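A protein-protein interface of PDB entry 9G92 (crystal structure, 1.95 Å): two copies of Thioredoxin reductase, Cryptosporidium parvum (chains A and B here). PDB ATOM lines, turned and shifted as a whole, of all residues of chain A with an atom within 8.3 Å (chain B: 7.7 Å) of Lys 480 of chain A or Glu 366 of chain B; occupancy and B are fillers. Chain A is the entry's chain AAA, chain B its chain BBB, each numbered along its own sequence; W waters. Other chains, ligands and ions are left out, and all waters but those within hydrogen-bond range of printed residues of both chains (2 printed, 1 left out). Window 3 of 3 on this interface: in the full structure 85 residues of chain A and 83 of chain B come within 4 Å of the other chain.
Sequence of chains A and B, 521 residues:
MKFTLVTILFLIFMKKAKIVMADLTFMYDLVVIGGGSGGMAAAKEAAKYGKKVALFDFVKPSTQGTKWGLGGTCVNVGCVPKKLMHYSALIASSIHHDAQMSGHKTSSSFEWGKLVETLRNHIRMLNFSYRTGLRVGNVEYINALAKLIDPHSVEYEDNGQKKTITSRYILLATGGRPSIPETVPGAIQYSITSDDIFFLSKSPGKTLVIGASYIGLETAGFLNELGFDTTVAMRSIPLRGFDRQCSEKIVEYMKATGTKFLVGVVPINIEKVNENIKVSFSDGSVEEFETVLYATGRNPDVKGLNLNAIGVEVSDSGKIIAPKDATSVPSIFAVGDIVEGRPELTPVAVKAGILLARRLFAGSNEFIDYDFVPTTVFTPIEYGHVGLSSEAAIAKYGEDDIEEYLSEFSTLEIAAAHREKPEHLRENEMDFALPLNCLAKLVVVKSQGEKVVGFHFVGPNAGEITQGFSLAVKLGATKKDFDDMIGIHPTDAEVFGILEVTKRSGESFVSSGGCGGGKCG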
ATOM      1  N   TYR A 405      -8.540  17.030 -17.067  1.00  0.00           N
ATOM      2  CA  TYR A 405      -8.080  15.960 -17.982  1.00  0.00           C
ATOM      3  C   TYR A 405      -8.320  16.428 -19.413  1.00  0.00           C
ATOM      4  O   TYR A 405      -9.432  16.929 -19.684  1.00  0.00           O
ATOM      5  CB  TYR A 405      -8.839  14.662 -17.735  1.00  0.00           C
ATOM      6  CG  TYR A 405      -8.626  14.038 -16.382  1.00  0.00           C
ATOM      7  CD1 TYR A 405      -9.364  14.443 -15.276  1.00  0.00           C
ATOM      8  CD2 TYR A 405      -7.727  12.995 -16.222  1.00  0.00           C
ATOM      9  CE1 TYR A 405      -9.201  13.840 -14.032  1.00  0.00           C
ATOM     10  CE2 TYR A 405      -7.551  12.376 -14.986  1.00  0.00           C
ATOM     11  CZ  TYR A 405      -8.269  12.818 -13.886  1.00  0.00           C
ATOM     12  OH  TYR A 405      -8.081  12.233 -12.671  1.00  0.00           O
ATOM     13  N   LEU A 442     -12.129  17.795 -19.506  1.00  0.00           N
ATOM     14  CA  LEU A 442     -13.077  17.628 -18.385  1.00  0.00           C
ATOM     15  C   LEU A 442     -12.453  18.333 -17.177  1.00  0.00           C
ATOM     16  O   LEU A 442     -11.244  18.171 -16.963  1.00  0.00           O
ATOM     17  CB  LEU A 442     -13.321  16.147 -18.079  1.00  0.00           C
ATOM     18  CG  LEU A 442     -14.097  15.333 -19.105  1.00  0.00           C
ATOM     19  CD1 LEU A 442     -14.121  13.868 -18.663  1.00  0.00           C
ATOM     20  CD2 LEU A 442     -15.498  15.893 -19.338  1.00  0.00           C
ATOM     21  N   VAL A 444     -12.926  18.635 -13.134  1.00  0.00           N
ATOM     22  CA  VAL A 444     -13.533  17.791 -12.074  1.00  0.00           C
ATOM     23  C   VAL A 444     -13.086  18.288 -10.688  1.00  0.00           C
ATOM     24  O   VAL A 444     -12.017  18.915 -10.569  1.00  0.00           O
ATOM     25  CB  VAL A 444     -13.188  16.304 -12.285  1.00  0.00           C
ATOM     26  CG1 VAL A 444     -13.504  15.867 -13.712  1.00  0.00           C
ATOM     27  CG2 VAL A 444     -11.747  15.979 -11.956  1.00  0.00           C
ATOM     28  N   GLY A 449     -15.293  13.292  -5.438  1.00  0.00           N
ATOM     29  CA  GLY A 449     -15.050  12.045  -6.194  1.00  0.00           C
ATOM     30  C   GLY A 449     -14.901  12.323  -7.691  1.00  0.00           C
ATOM     31  O   GLY A 449     -15.441  11.547  -8.504  1.00  0.00           O
ATOM     32  N   GLU A 450     -14.180  13.387  -8.027  1.00  0.00           N
ATOM     33  CA  GLU A 450     -13.953  13.893  -9.413  1.00  0.00           C
ATOM     34  C   GLU A 450     -15.297  14.044 -10.126  1.00  0.00           C
ATOM     35  O   GLU A 450     -15.407  13.616 -11.283  1.00  0.00           O
ATOM     36  CB  GLU A 450     -12.977  12.975 -10.149  1.00  0.00           C
ATOM     37  CG  GLU A 450     -11.563  13.034  -9.600  1.00  0.00           C
ATOM     38  CD  GLU A 450     -10.555  12.334 -10.481  1.00  0.00           C
ATOM     39  OE1 GLU A 450     -10.836  11.187 -10.869  1.00  0.00           O
ATOM     40  OE2 GLU A 450      -9.525  12.939 -10.807  1.00  0.00           O
ATOM     41  N   LYS A 451     -16.283  14.652  -9.468  1.00  0.00           N
ATOM     42  CA  LYS A 451     -17.533  15.060 -10.142  1.00  0.00           C
ATOM     43  C   LYS A 451     -17.165  16.037 -11.276  1.00  0.00           C
ATOM     44  O   LYS A 451     -16.311  16.931 -11.053  1.00  0.00           O
ATOM     45  CB  LYS A 451     -18.491  15.729  -9.156  1.00  0.00           C
ATOM     46  CG  LYS A 451     -19.926  15.771  -9.642  1.00  0.00           C
ATOM     47  CD  LYS A 451     -20.761  16.781  -8.916  1.00  0.00           C
ATOM     48  CE  LYS A 451     -22.220  16.462  -9.112  1.00  0.00           C
ATOM     49  NZ  LYS A 451     -23.095  17.337  -8.303  1.00  0.00           N
ATOM     50  N   VAL A 452     -17.758  15.862 -12.459  1.00  0.00           N
ATOM     51  CA  VAL A 452     -17.493  16.758 -13.622  1.00  0.00           C
ATOM     52  C   VAL A 452     -18.282  18.056 -13.418  1.00  0.00           C
ATOM     53  O   VAL A 452     -19.470  17.981 -13.353  1.00  0.00           O
ATOM     54  CB  VAL A 452     -17.839  16.079 -14.972  1.00  0.00           C
ATOM     55  CG1 VAL A 452     -17.648  17.026 -16.159  1.00  0.00           C
ATOM     56  CG2 VAL A 452     -17.013  14.823 -15.165  1.00  0.00           C
ATOM     57  N   ALA A 477     -22.503  13.269 -13.502  1.00  0.00           N
ATOM     58  CA  ALA A 477     -21.478  12.300 -13.953  1.00  0.00           C
ATOM     59  C   ALA A 477     -20.153  12.595 -13.270  1.00  0.00           C
ATOM     60  O   ALA A 477     -19.811  13.785 -13.113  1.00  0.00           O
ATOM     61  CB  ALA A 477     -21.350  12.341 -15.454  1.00  0.00           C
ATOM     62  N   THR A 478     -19.398  11.545 -12.919  1.00  0.00           N
ATOM     63  CA  THR A 478     -18.023  11.643 -12.365  1.00  0.00           C
ATOM     64  C   THR A 478     -17.014  11.247 -13.439  1.00  0.00           C
ATOM     65  O   THR A 478     -17.448  10.663 -14.422  1.00  0.00           O
ATOM     66  CB  THR A 478     -17.836  10.702 -11.166  1.00  0.00           C
ATOM     67  OG1 THR A 478     -17.875   9.361 -11.697  1.00  0.00           O
ATOM     68  CG2 THR A 478     -18.879  10.907 -10.086  1.00  0.00           C
ATOM     69  N   LYS A 479     -15.722  11.504 -13.210  1.00  0.00           N
ATOM     70  CA  LYS A 479     -14.628  11.004 -14.084  1.00  0.00           C
ATOM     71  C   LYS A 479     -14.773   9.491 -14.290  1.00  0.00           C
ATOM     72  O   LYS A 479     -14.570   9.004 -15.429  1.00  0.00           O
ATOM     73  CB  LYS A 479     -13.255  11.350 -13.522  1.00  0.00           C
ATOM     74  CG  LYS A 479     -12.100  11.039 -14.467  1.00  0.00           C
ATOM     75  CD  LYS A 479     -12.327  11.467 -15.895  1.00  0.00           C
ATOM     76  CE  LYS A 479     -11.038  11.594 -16.673  1.00  0.00           C
ATOM     77  NZ  LYS A 479     -10.380  10.291 -16.858  1.00  0.00           N
ATOM     78  N   LYS A 480     -15.099   8.752 -13.231  1.00  0.00           N
ATOM     79  CA  LYS A 480     -15.247   7.286 -13.310  1.00  0.00           C
ATOM     80  C   LYS A 480     -16.375   6.919 -14.288  1.00  0.00           C
ATOM     81  O   LYS A 480     -16.195   5.955 -15.047  1.00  0.00           O
ATOM     82  CB  LYS A 480     -15.479   6.663 -11.934  1.00  0.00           C
ATOM     83  CG  LYS A 480     -15.647   5.155 -11.990  1.00  0.00           C
ATOM     84  CD  LYS A 480     -15.831   4.508 -10.617  1.00  0.00           C
ATOM     85  CE  LYS A 480     -16.216   3.042 -10.702  1.00  0.00           C
ATOM     86  NZ  LYS A 480     -15.372   2.303 -11.678  1.00  0.00           N
ATOM     87  N   ASP A 481     -17.500   7.619 -14.267  1.00  0.00           N
ATOM     88  CA  ASP A 481     -18.610   7.353 -15.216  1.00  0.00           C
ATOM     89  C   ASP A 481     -18.111   7.563 -16.653  1.00  0.00           C
ATOM     90  O   ASP A 481     -18.450   6.751 -17.502  1.00  0.00           O
ATOM     91  CB  ASP A 481     -19.819   8.235 -14.956  1.00  0.00           C
ATOM     92  CG  ASP A 481     -20.475   8.023 -13.596  1.00  0.00           C
ATOM     93  OD1 ASP A 481     -20.522   6.863 -13.142  1.00  0.00           O
ATOM     94  OD2 ASP A 481     -20.918   9.035 -13.016  1.00  0.00           O
ATOM     95  N   PHE A 482     -17.336   8.617 -16.911  1.00  0.00           N
ATOM     96  CA  PHE A 482     -16.734   8.864 -18.246  1.00  0.00           C
ATOM     97  C   PHE A 482     -15.770   7.730 -18.614  1.00  0.00           C
ATOM     98  O   PHE A 482     -15.810   7.249 -19.772  1.00  0.00           O
ATOM     99  CB  PHE A 482     -16.055  10.228 -18.263  1.00  0.00           C
ATOM    100  CG  PHE A 482     -16.975  11.383 -18.544  1.00  0.00           C
ATOM    101  CD1 PHE A 482     -17.770  11.923 -17.556  1.00  0.00           C
ATOM    102  CD2 PHE A 482     -17.047  11.918 -19.820  1.00  0.00           C
ATOM    103  CE1 PHE A 482     -18.604  12.995 -17.821  1.00  0.00           C
ATOM    104  CE2 PHE A 482     -17.894  12.978 -20.094  1.00  0.00           C
ATOM    105  CZ  PHE A 482     -18.670  13.527 -19.089  1.00  0.00           C
ATOM    106  N   ASP A 483     -14.930   7.296 -17.677  1.00  0.00           N
ATOM    107  CA  ASP A 483     -13.881   6.267 -17.928  1.00  0.00           C
ATOM    108  C   ASP A 483     -14.507   4.899 -18.217  1.00  0.00           C
ATOM    109  O   ASP A 483     -13.862   4.094 -18.922  1.00  0.00           O
ATOM    110  CB  ASP A 483     -12.918   6.133 -16.749  1.00  0.00           C
ATOM    111  CG  ASP A 483     -11.996   7.320 -16.522  1.00  0.00           C
ATOM    112  OD1 ASP A 483     -11.816   8.144 -17.451  1.00  0.00           O
ATOM    113  OD2 ASP A 483     -11.393   7.370 -15.443  1.00  0.00           O
ATOM    114  N   ASP A 484     -15.685   4.635 -17.663  1.00  0.00           N
ATOM    115  CA  ASP A 484     -16.405   3.336 -17.768  1.00  0.00           C
ATOM    116  C   ASP A 484     -17.408   3.403 -18.924  1.00  0.00           C
ATOM    117  O   ASP A 484     -18.046   2.371 -19.229  1.00  0.00           O
ATOM    118  CB  ASP A 484     -17.087   2.989 -16.436  1.00  0.00           C
ATOM    119  CG  ASP A 484     -16.084   2.690 -15.321  1.00  0.00           C
ATOM    120  OD1 ASP A 484     -14.916   2.526 -15.634  1.00  0.00           O
ATOM    121  OD2 ASP A 484     -16.496   2.681 -14.151  1.00  0.00           O
ATOM    122  N   MET A 485     -17.565   4.571 -19.555  1.00  0.00           N
ATOM    123  CA  MET A 485     -18.457   4.703 -20.737  1.00  0.00           C
ATOM    124  C   MET A 485     -17.803   3.957 -21.911  1.00  0.00           C
ATOM    125  O   MET A 485     -16.651   4.258 -22.228  1.00  0.00           O
ATOM    126  CB  MET A 485     -18.597   6.188 -21.073  1.00  0.00           C
ATOM    127  CG  MET A 485     -19.406   6.494 -22.291  1.00  0.00           C
ATOM    128  SD  MET A 485     -19.397   8.287 -22.582  1.00  0.00           S
ATOM    129  CE  MET A 485     -17.666   8.571 -22.960  1.00  0.00           C
ATOM    130  N   PHE A 496     -13.867  11.124 -24.842  1.00  0.00           N
ATOM    131  CA  PHE A 496     -14.276  11.445 -23.458  1.00  0.00           C
ATOM    132  C   PHE A 496     -14.276  10.181 -22.589  1.00  0.00           C
ATOM    133  O   PHE A 496     -14.285  10.343 -21.356  1.00  0.00           O
ATOM    134  CB  PHE A 496     -15.604  12.188 -23.450  1.00  0.00           C
ATOM    135  CG  PHE A 496     -15.433  13.644 -23.821  1.00  0.00           C
ATOM    136  CD1 PHE A 496     -14.868  14.550 -22.943  1.00  0.00           C
ATOM    137  CD2 PHE A 496     -15.789  14.092 -25.075  1.00  0.00           C
ATOM    138  CE1 PHE A 496     -14.740  15.896 -23.270  1.00  0.00           C
ATOM    139  CE2 PHE A 496     -15.606  15.422 -25.430  1.00  0.00           C
ATOM    140  CZ  PHE A 496     -15.079  16.322 -24.531  1.00  0.00           C
ATOM    141  N   GLY A 497     -14.181   8.999 -23.197  1.00  0.00           N
ATOM    142  CA  GLY A 497     -14.071   7.730 -22.443  1.00  0.00           C
ATOM    143  C   GLY A 497     -12.641   7.386 -22.066  1.00  0.00           C
ATOM    144  O   GLY A 497     -12.468   6.428 -21.313  1.00  0.00           O
ATOM    145  N   LYS B 324     -17.155 -14.417 -18.935  1.00  0.00           N
ATOM    146  CA  LYS B 324     -16.399 -13.495 -18.046  1.00  0.00           C
ATOM    147  C   LYS B 324     -14.947 -13.454 -18.512  1.00  0.00           C
ATOM    148  O   LYS B 324     -14.099 -13.102 -17.686  1.00  0.00           O
ATOM    149  CB  LYS B 324     -16.517 -13.918 -16.579  1.00  0.00           C
ATOM    150  CG  LYS B 324     -17.953 -14.083 -16.077  1.00  0.00           C
ATOM    151  CD  LYS B 324     -18.031 -14.647 -14.673  1.00  0.00           C
ATOM    152  CE  LYS B 324     -19.109 -13.994 -13.833  1.00  0.00           C
ATOM    153  NZ  LYS B 324     -18.700 -12.627 -13.417  1.00  0.00           N
ATOM    154  N   ASP B 325     -14.713 -13.762 -19.805  1.00  0.00           N
ATOM    155  CA  ASP B 325     -13.392 -13.770 -20.490  1.00  0.00           C
ATOM    156  C   ASP B 325     -12.560 -15.020 -20.149  1.00  0.00           C
ATOM    157  O   ASP B 325     -11.562 -15.218 -20.845  1.00  0.00           O
ATOM    158  CB  ASP B 325     -12.571 -12.519 -20.190  1.00  0.00           C
ATOM    159  CG  ASP B 325     -13.288 -11.192 -20.362  1.00  0.00           C
ATOM    160  OD1 ASP B 325     -14.205 -11.067 -21.234  1.00  0.00           O
ATOM    161  OD2 ASP B 325     -12.902 -10.282 -19.646  1.00  0.00           O
ATOM    162  N   LYS B 351     -11.828  -2.464 -24.277  1.00  0.00           N
ATOM    163  CA  LYS B 351     -12.115  -2.323 -22.832  1.00  0.00           C
ATOM    164  C   LYS B 351     -12.019  -3.711 -22.145  1.00  0.00           C
ATOM    165  O   LYS B 351     -11.477  -3.786 -21.061  1.00  0.00           O
ATOM    166  CB  LYS B 351     -13.476  -1.674 -22.558  1.00  0.00           C
ATOM    167  CG  LYS B 351     -13.626  -1.365 -21.077  1.00  0.00           C
ATOM    168  CD  LYS B 351     -14.733  -0.413 -20.707  1.00  0.00           C
ATOM    169  CE  LYS B 351     -14.539   0.995 -21.240  1.00  0.00           C
ATOM    170  NZ  LYS B 351     -13.397   1.686 -20.595  1.00  0.00           N
ATOM    171  N   ALA B 352     -12.504  -4.772 -22.776  1.00  0.00           N
ATOM    172  CA  ALA B 352     -12.408  -6.148 -22.222  1.00  0.00           C
ATOM    173  C   ALA B 352     -10.939  -6.505 -21.999  1.00  0.00           C
ATOM    174  O   ALA B 352     -10.637  -6.944 -20.899  1.00  0.00           O
ATOM    175  CB  ALA B 352     -13.128  -7.150 -23.085  1.00  0.00           C
ATOM    176  N   ILE B 354      -8.302  -4.499 -21.547  1.00  0.00           N
ATOM    177  CA  ILE B 354      -7.715  -3.626 -20.491  1.00  0.00           C
ATOM    178  C   ILE B 354      -8.192  -4.149 -19.127  1.00  0.00           C
ATOM    179  O   ILE B 354      -7.314  -4.305 -18.207  1.00  0.00           O
ATOM    180  CB  ILE B 354      -8.055  -2.138 -20.731  1.00  0.00           C
ATOM    181  CG1 ILE B 354      -7.341  -1.577 -21.968  1.00  0.00           C
ATOM    182  CG2 ILE B 354      -7.734  -1.302 -19.497  1.00  0.00           C
ATOM    183  CD1 ILE B 354      -7.791  -0.160 -22.335  1.00  0.00           C
ATOM    184  N   LEU B 355      -9.504  -4.368 -18.968  1.00  0.00           N
ATOM    185  CA  LEU B 355     -10.076  -4.774 -17.659  1.00  0.00           C
ATOM    186  C   LEU B 355      -9.561  -6.176 -17.326  1.00  0.00           C
ATOM    187  O   LEU B 355      -9.262  -6.417 -16.155  1.00  0.00           O
ATOM    188  CB  LEU B 355     -11.603  -4.717 -17.644  1.00  0.00           C
ATOM    189  CG  LEU B 355     -12.239  -3.339 -17.815  1.00  0.00           C
ATOM    190  CD1 LEU B 355     -13.753  -3.443 -17.759  1.00  0.00           C
ATOM    191  CD2 LEU B 355     -11.734  -2.334 -16.795  1.00  0.00           C
ATOM    192  N   LEU B 356      -9.392  -7.048 -18.319  1.00  0.00           N
ATOM    193  CA  LEU B 356      -8.817  -8.402 -18.068  1.00  0.00           C
ATOM    194  C   LEU B 356      -7.420  -8.229 -17.474  1.00  0.00           C
ATOM    195  O   LEU B 356      -7.148  -8.854 -16.454  1.00  0.00           O
ATOM    196  CB  LEU B 356      -8.799  -9.244 -19.341  1.00  0.00           C
ATOM    197  CG  LEU B 356      -8.044 -10.560 -19.223  1.00  0.00           C
ATOM    198  CD1 LEU B 356      -8.706 -11.460 -18.202  1.00  0.00           C
ATOM    199  CD2 LEU B 356      -7.924 -11.251 -20.563  1.00  0.00           C
ATOM    200  N   ARG B 358      -6.131  -5.792 -15.808  1.00  0.00           N
ATOM    201  CA  ARG B 358      -6.259  -5.257 -14.439  1.00  0.00           C
ATOM    202  C   ARG B 358      -6.772  -6.333 -13.462  1.00  0.00           C
ATOM    203  O   ARG B 358      -6.366  -6.295 -12.310  1.00  0.00           O
ATOM    204  CB  ARG B 358      -7.184  -4.044 -14.424  1.00  0.00           C
ATOM    205  CG  ARG B 358      -6.604  -2.848 -15.154  1.00  0.00           C
ATOM    206  CD  ARG B 358      -7.594  -1.697 -15.205  1.00  0.00           C
ATOM    207  NE  ARG B 358      -7.077  -0.603 -16.014  1.00  0.00           N
ATOM    208  CZ  ARG B 358      -7.781   0.484 -16.336  1.00  0.00           C
ATOM    209  NH1 ARG B 358      -9.026   0.622 -15.909  1.00  0.00           N
ATOM    210  NH2 ARG B 358      -7.237   1.433 -17.083  1.00  0.00           N
ATOM    211  N   ARG B 359      -7.669  -7.220 -13.876  1.00  0.00           N
ATOM    212  CA  ARG B 359      -8.170  -8.320 -13.003  1.00  0.00           C
ATOM    213  C   ARG B 359      -7.028  -9.315 -12.787  1.00  0.00           C
ATOM    214  O   ARG B 359      -6.888  -9.803 -11.668  1.00  0.00           O
ATOM    215  CB  ARG B 359      -9.420  -8.981 -13.608  1.00  0.00           C
ATOM    216  CG  ARG B 359     -10.639  -8.067 -13.683  1.00  0.00           C
ATOM    217  CD  ARG B 359     -11.946  -8.834 -13.731  1.00  0.00           C
ATOM    218  NE  ARG B 359     -11.858  -9.774 -14.833  1.00  0.00           N
ATOM    219  CZ  ARG B 359     -12.098  -9.474 -16.100  1.00  0.00           C
ATOM    220  NH1 ARG B 359     -12.485  -8.253 -16.446  1.00  0.00           N
ATOM    221  NH2 ARG B 359     -11.916 -10.393 -17.030  1.00  0.00           N
ATOM    222  N   GLY B 363      -5.643  -6.834  -9.264  1.00  0.00           N
ATOM    223  CA  GLY B 363      -6.709  -7.155  -8.291  1.00  0.00           C
ATOM    224  C   GLY B 363      -8.000  -6.430  -8.586  1.00  0.00           C
ATOM    225  O   GLY B 363      -8.811  -6.296  -7.670  1.00  0.00           O
ATOM    226  N   SER B 364      -8.228  -6.015  -9.832  1.00  0.00           N
ATOM    227  CA  SER B 364      -9.510  -5.379 -10.232  1.00  0.00           C
ATOM    228  C   SER B 364     -10.626  -6.428 -10.208  1.00  0.00           C
ATOM    229  O   SER B 364     -10.348  -7.605 -10.492  1.00  0.00           O
ATOM    230  CB  SER B 364      -9.411  -4.732 -11.603  1.00  0.00           C
ATOM    231  OG  SER B 364     -10.669  -4.195 -11.984  1.00  0.00           O
ATOM    232  N   ASN B 365     -11.861  -5.998  -9.948  1.00  0.00           N
ATOM    233  CA  ASN B 365     -13.093  -6.814 -10.114  1.00  0.00           C
ATOM    234  C   ASN B 365     -13.981  -6.229 -11.202  1.00  0.00           C
ATOM    235  O   ASN B 365     -15.127  -6.656 -11.303  1.00  0.00           O
ATOM    236  CB  ASN B 365     -13.844  -6.980  -8.789  1.00  0.00           C
ATOM    237  CG  ASN B 365     -13.103  -7.946  -7.892  1.00  0.00           C
ATOM    238  OD1 ASN B 365     -12.977  -9.118  -8.230  1.00  0.00           O
ATOM    239  ND2 ASN B 365     -12.560  -7.463  -6.789  1.00  0.00           N
ATOM    240  N   GLU B 366     -13.449  -5.369 -12.064  1.00  0.00           N
ATOM    241  CA  GLU B 366     -14.275  -4.605 -13.045  1.00  0.00           C
ATOM    242  C   GLU B 366     -14.523  -5.429 -14.312  1.00  0.00           C
ATOM    243  O   GLU B 366     -13.580  -6.057 -14.837  1.00  0.00           O
ATOM    244  CB  GLU B 366     -13.613  -3.256 -13.339  1.00  0.00           C
ATOM    245  CG  GLU B 366     -13.510  -2.405 -12.087  1.00  0.00           C
ATOM    246  CD  GLU B 366     -13.803  -0.910 -12.224  1.00  0.00           C
ATOM    247  OE1 GLU B 366     -13.133  -0.118 -11.521  1.00  0.00           O
ATOM    248  OE2 GLU B 366     -14.725  -0.544 -12.997  1.00  0.00           O
ATOM    249  N   PHE B 367     -15.779  -5.411 -14.754  1.00  0.00           N
ATOM    250  CA  PHE B 367     -16.287  -5.988 -16.013  1.00  0.00           C
ATOM    251  C   PHE B 367     -17.073  -4.910 -16.753  1.00  0.00           C
ATOM    252  O   PHE B 367     -17.687  -4.040 -16.118  1.00  0.00           O
ATOM    253  CB  PHE B 367     -17.182  -7.202 -15.750  1.00  0.00           C
ATOM    254  CG  PHE B 367     -16.435  -8.417 -15.241  1.00  0.00           C
ATOM    255  CD1 PHE B 367     -16.247  -8.604 -13.881  1.00  0.00           C
ATOM    256  CD2 PHE B 367     -15.901  -9.354 -16.120  1.00  0.00           C
ATOM    257  CE1 PHE B 367     -15.561  -9.711 -13.397  1.00  0.00           C
ATOM    258  CE2 PHE B 367     -15.202 -10.451 -15.632  1.00  0.00           C
ATOM    259  CZ  PHE B 367     -15.039 -10.635 -14.276  1.00  0.00           C
ATOM    260  N   ILE B 368     -17.099  -5.010 -18.074  1.00  0.00           N
ATOM    261  CA  ILE B 368     -18.014  -4.187 -18.910  1.00  0.00           C
ATOM    262  C   ILE B 368     -19.461  -4.441 -18.477  1.00  0.00           C
ATOM    263  O   ILE B 368     -19.827  -5.606 -18.290  1.00  0.00           O
ATOM    264  CB  ILE B 368     -17.838  -4.547 -20.386  1.00  0.00           C
ATOM    265  CG1 ILE B 368     -16.486  -4.051 -20.906  1.00  0.00           C
ATOM    266  CG2 ILE B 368     -19.019  -4.032 -21.214  1.00  0.00           C
ATOM    267  CD1 ILE B 368     -16.125  -4.645 -22.235  1.00  0.00           C
ATOM    268  N   ASP B 369     -20.264  -3.387 -18.415  1.00  0.00           N
ATOM    269  CA  ASP B 369     -21.732  -3.491 -18.283  1.00  0.00           C
ATOM    270  C   ASP B 369     -22.322  -3.586 -19.688  1.00  0.00           C
ATOM    271  O   ASP B 369     -22.415  -2.526 -20.343  1.00  0.00           O
ATOM    272  CB  ASP B 369     -22.264  -2.320 -17.464  1.00  0.00           C
ATOM    273  CG  ASP B 369     -23.766  -2.408 -17.249  1.00  0.00           C
ATOM    274  OD1 ASP B 369     -24.410  -3.298 -17.862  1.00  0.00           O
ATOM    275  OD2 ASP B 369     -24.282  -1.546 -16.505  1.00  0.00           O
ATOM    276  N   LEU B 471     -24.159   7.883 -22.151  1.00  0.00           N
ATOM    277  CA  LEU B 471     -23.793   8.076 -20.731  1.00  0.00           C
ATOM    278  C   LEU B 471     -25.010   8.563 -19.929  1.00  0.00           C
ATOM    279  O   LEU B 471     -25.248   7.999 -18.855  1.00  0.00           O
ATOM    280  CB  LEU B 471     -22.623   9.039 -20.621  1.00  0.00           C
ATOM    281  CG  LEU B 471     -22.108   9.260 -19.202  1.00  0.00           C
ATOM    282  CD1 LEU B 471     -21.654   7.952 -18.593  1.00  0.00           C
ATOM    283  CD2 LEU B 471     -20.973  10.267 -19.190  1.00  0.00           C
ATOM    284  N   LYS B 474     -27.244   5.513 -19.454  1.00  0.00           N
ATOM    285  CA  LYS B 474     -26.559   4.614 -18.494  1.00  0.00           C
ATOM    286  C   LYS B 474     -26.725   5.128 -17.064  1.00  0.00           C
ATOM    287  O   LYS B 474     -26.760   4.284 -16.158  1.00  0.00           O
ATOM    288  CB  LYS B 474     -25.087   4.478 -18.864  1.00  0.00           C
ATOM    289  CG  LYS B 474     -24.273   3.549 -17.987  1.00  0.00           C
ATOM    290  CD  LYS B 474     -22.900   3.290 -18.559  1.00  0.00           C
ATOM    291  CE  LYS B 474     -22.148   2.279 -17.736  1.00  0.00           C
ATOM    292  NZ  LYS B 474     -20.805   2.012 -18.284  1.00  0.00           N
HETATM  293  O   HOH W   1     -13.529   1.270 -17.756  1.00  0.00           O
HETATM  294  O   HOH W   2     -20.062   4.646 -17.328  1.00  0.00           O
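The side-chain amino group of Lys 351 of chain B sits at hydrogen-bond distance from the backbone carbonyl oxygen of Asp 483 of chain A (3.0 Å).
The backbone carbonyl oxygen (O) of Asp 484 of chain A sits at hydrogen-bond distance from the side-chain amino group (NZ) of Lys 474 of chain B, at 2.9 Å.
NZ of Lys 480 of chain A lies within salt-bridge range of OE2 of Glu 366 of chain B (3.2 Å).
The side-chain hydroxyl (OG) of Ser 364 of chain B sits at hydrogen-bond distance from the backbone NH (N) of Glu 366 of chain B, 3.0 Å away.
OD1 of Asp 483 of chain A lies within salt-bridge range of NZ of Lys 479 of chain A (2.7 Å).
NZ of Lys 480 of chain A lies within salt-bridge range of OD2 of Asp 484 of chain A, at 2.7 Å.
The side-chain carboxylate (OD2) of Asp 481 of chain A sits at hydrogen-bond distance from the backbone NH (N) of Thr 478 of chain A (2.9 Å).
The side-chain hydroxyl of Thr 478 of chain A sits close to the backbone NH of Lys 480 of chain A (3.2 Å).
The guanidinium group (NH1) of Arg 359 of chain B sits at hydrogen-bond distance from the backbone carbonyl oxygen (O) of Glu 366 of chain B, at 2.9 Å.
Among the printed residues, merely in contact across the chains: Asp 481 of chain A with Leu 471 of chain B (3.6 Å), Phe 482 of chain A with Leu 471 of chain B (3.9 Å), Asp 484 of chain A with Glu 366 of chain B (3.9 Å) and Met 485 of chain A with Leu 471 of chain B (3.8 Å).
Lys 480 of chain A touches just one residue of chain B: Glu 366 (3.2 Å).
Of the printed residues of chain B, Asp 481 of chain A touches Leu 471 (3.6 Å).
Of the printed residues of chain B, Met 485 of chain A touches Leu 471 (3.8 Å).
Leu 356 of chain B touches none of the printed residues of chain A.
Glu 366 of chain B touches just these residues of chain A: Lys 480 (3.2 Å) and Asp 484 (3.9 Å).
Printed residues of chain A within 4 Å of Leu 471 of chain B: Asp 481, Phe 482 and Met 485.
Of the printed residues of chain A, Lys 474 of chain B touches Asp 484 (2.9 Å).
The nearest residue of chain A that does not touch Glu 366 of chain B is Asp 483 of chain A (7.5 Å).
Hydrophobic or aromatic side chains of chain B that line the printed part of chain A: Leu 471.
Printed residues of chain A that touch a printed residue of chain B: Lys 480, Asp 481, Phe 482, Asp 483, Asp 484 and Met 485.
No position is printed for both chains.
Water W2 lies within hydrogen-bond range of the backbone carbonyl oxygen of Asp 481 of chain A (2.7 Å), the side-chain amino group of Lys 474 of chain B (2.9 Å) and the backbone NH of Met 485 of chain A (3.3 Å).
Water W1 lies within hydrogen-bond range of OD1 of Asp 484 of chain A (2.8 Å), NZ of Lys 351 of chain B (2.9 Å) and O of Asp 483 of chain A (3.1 Å).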
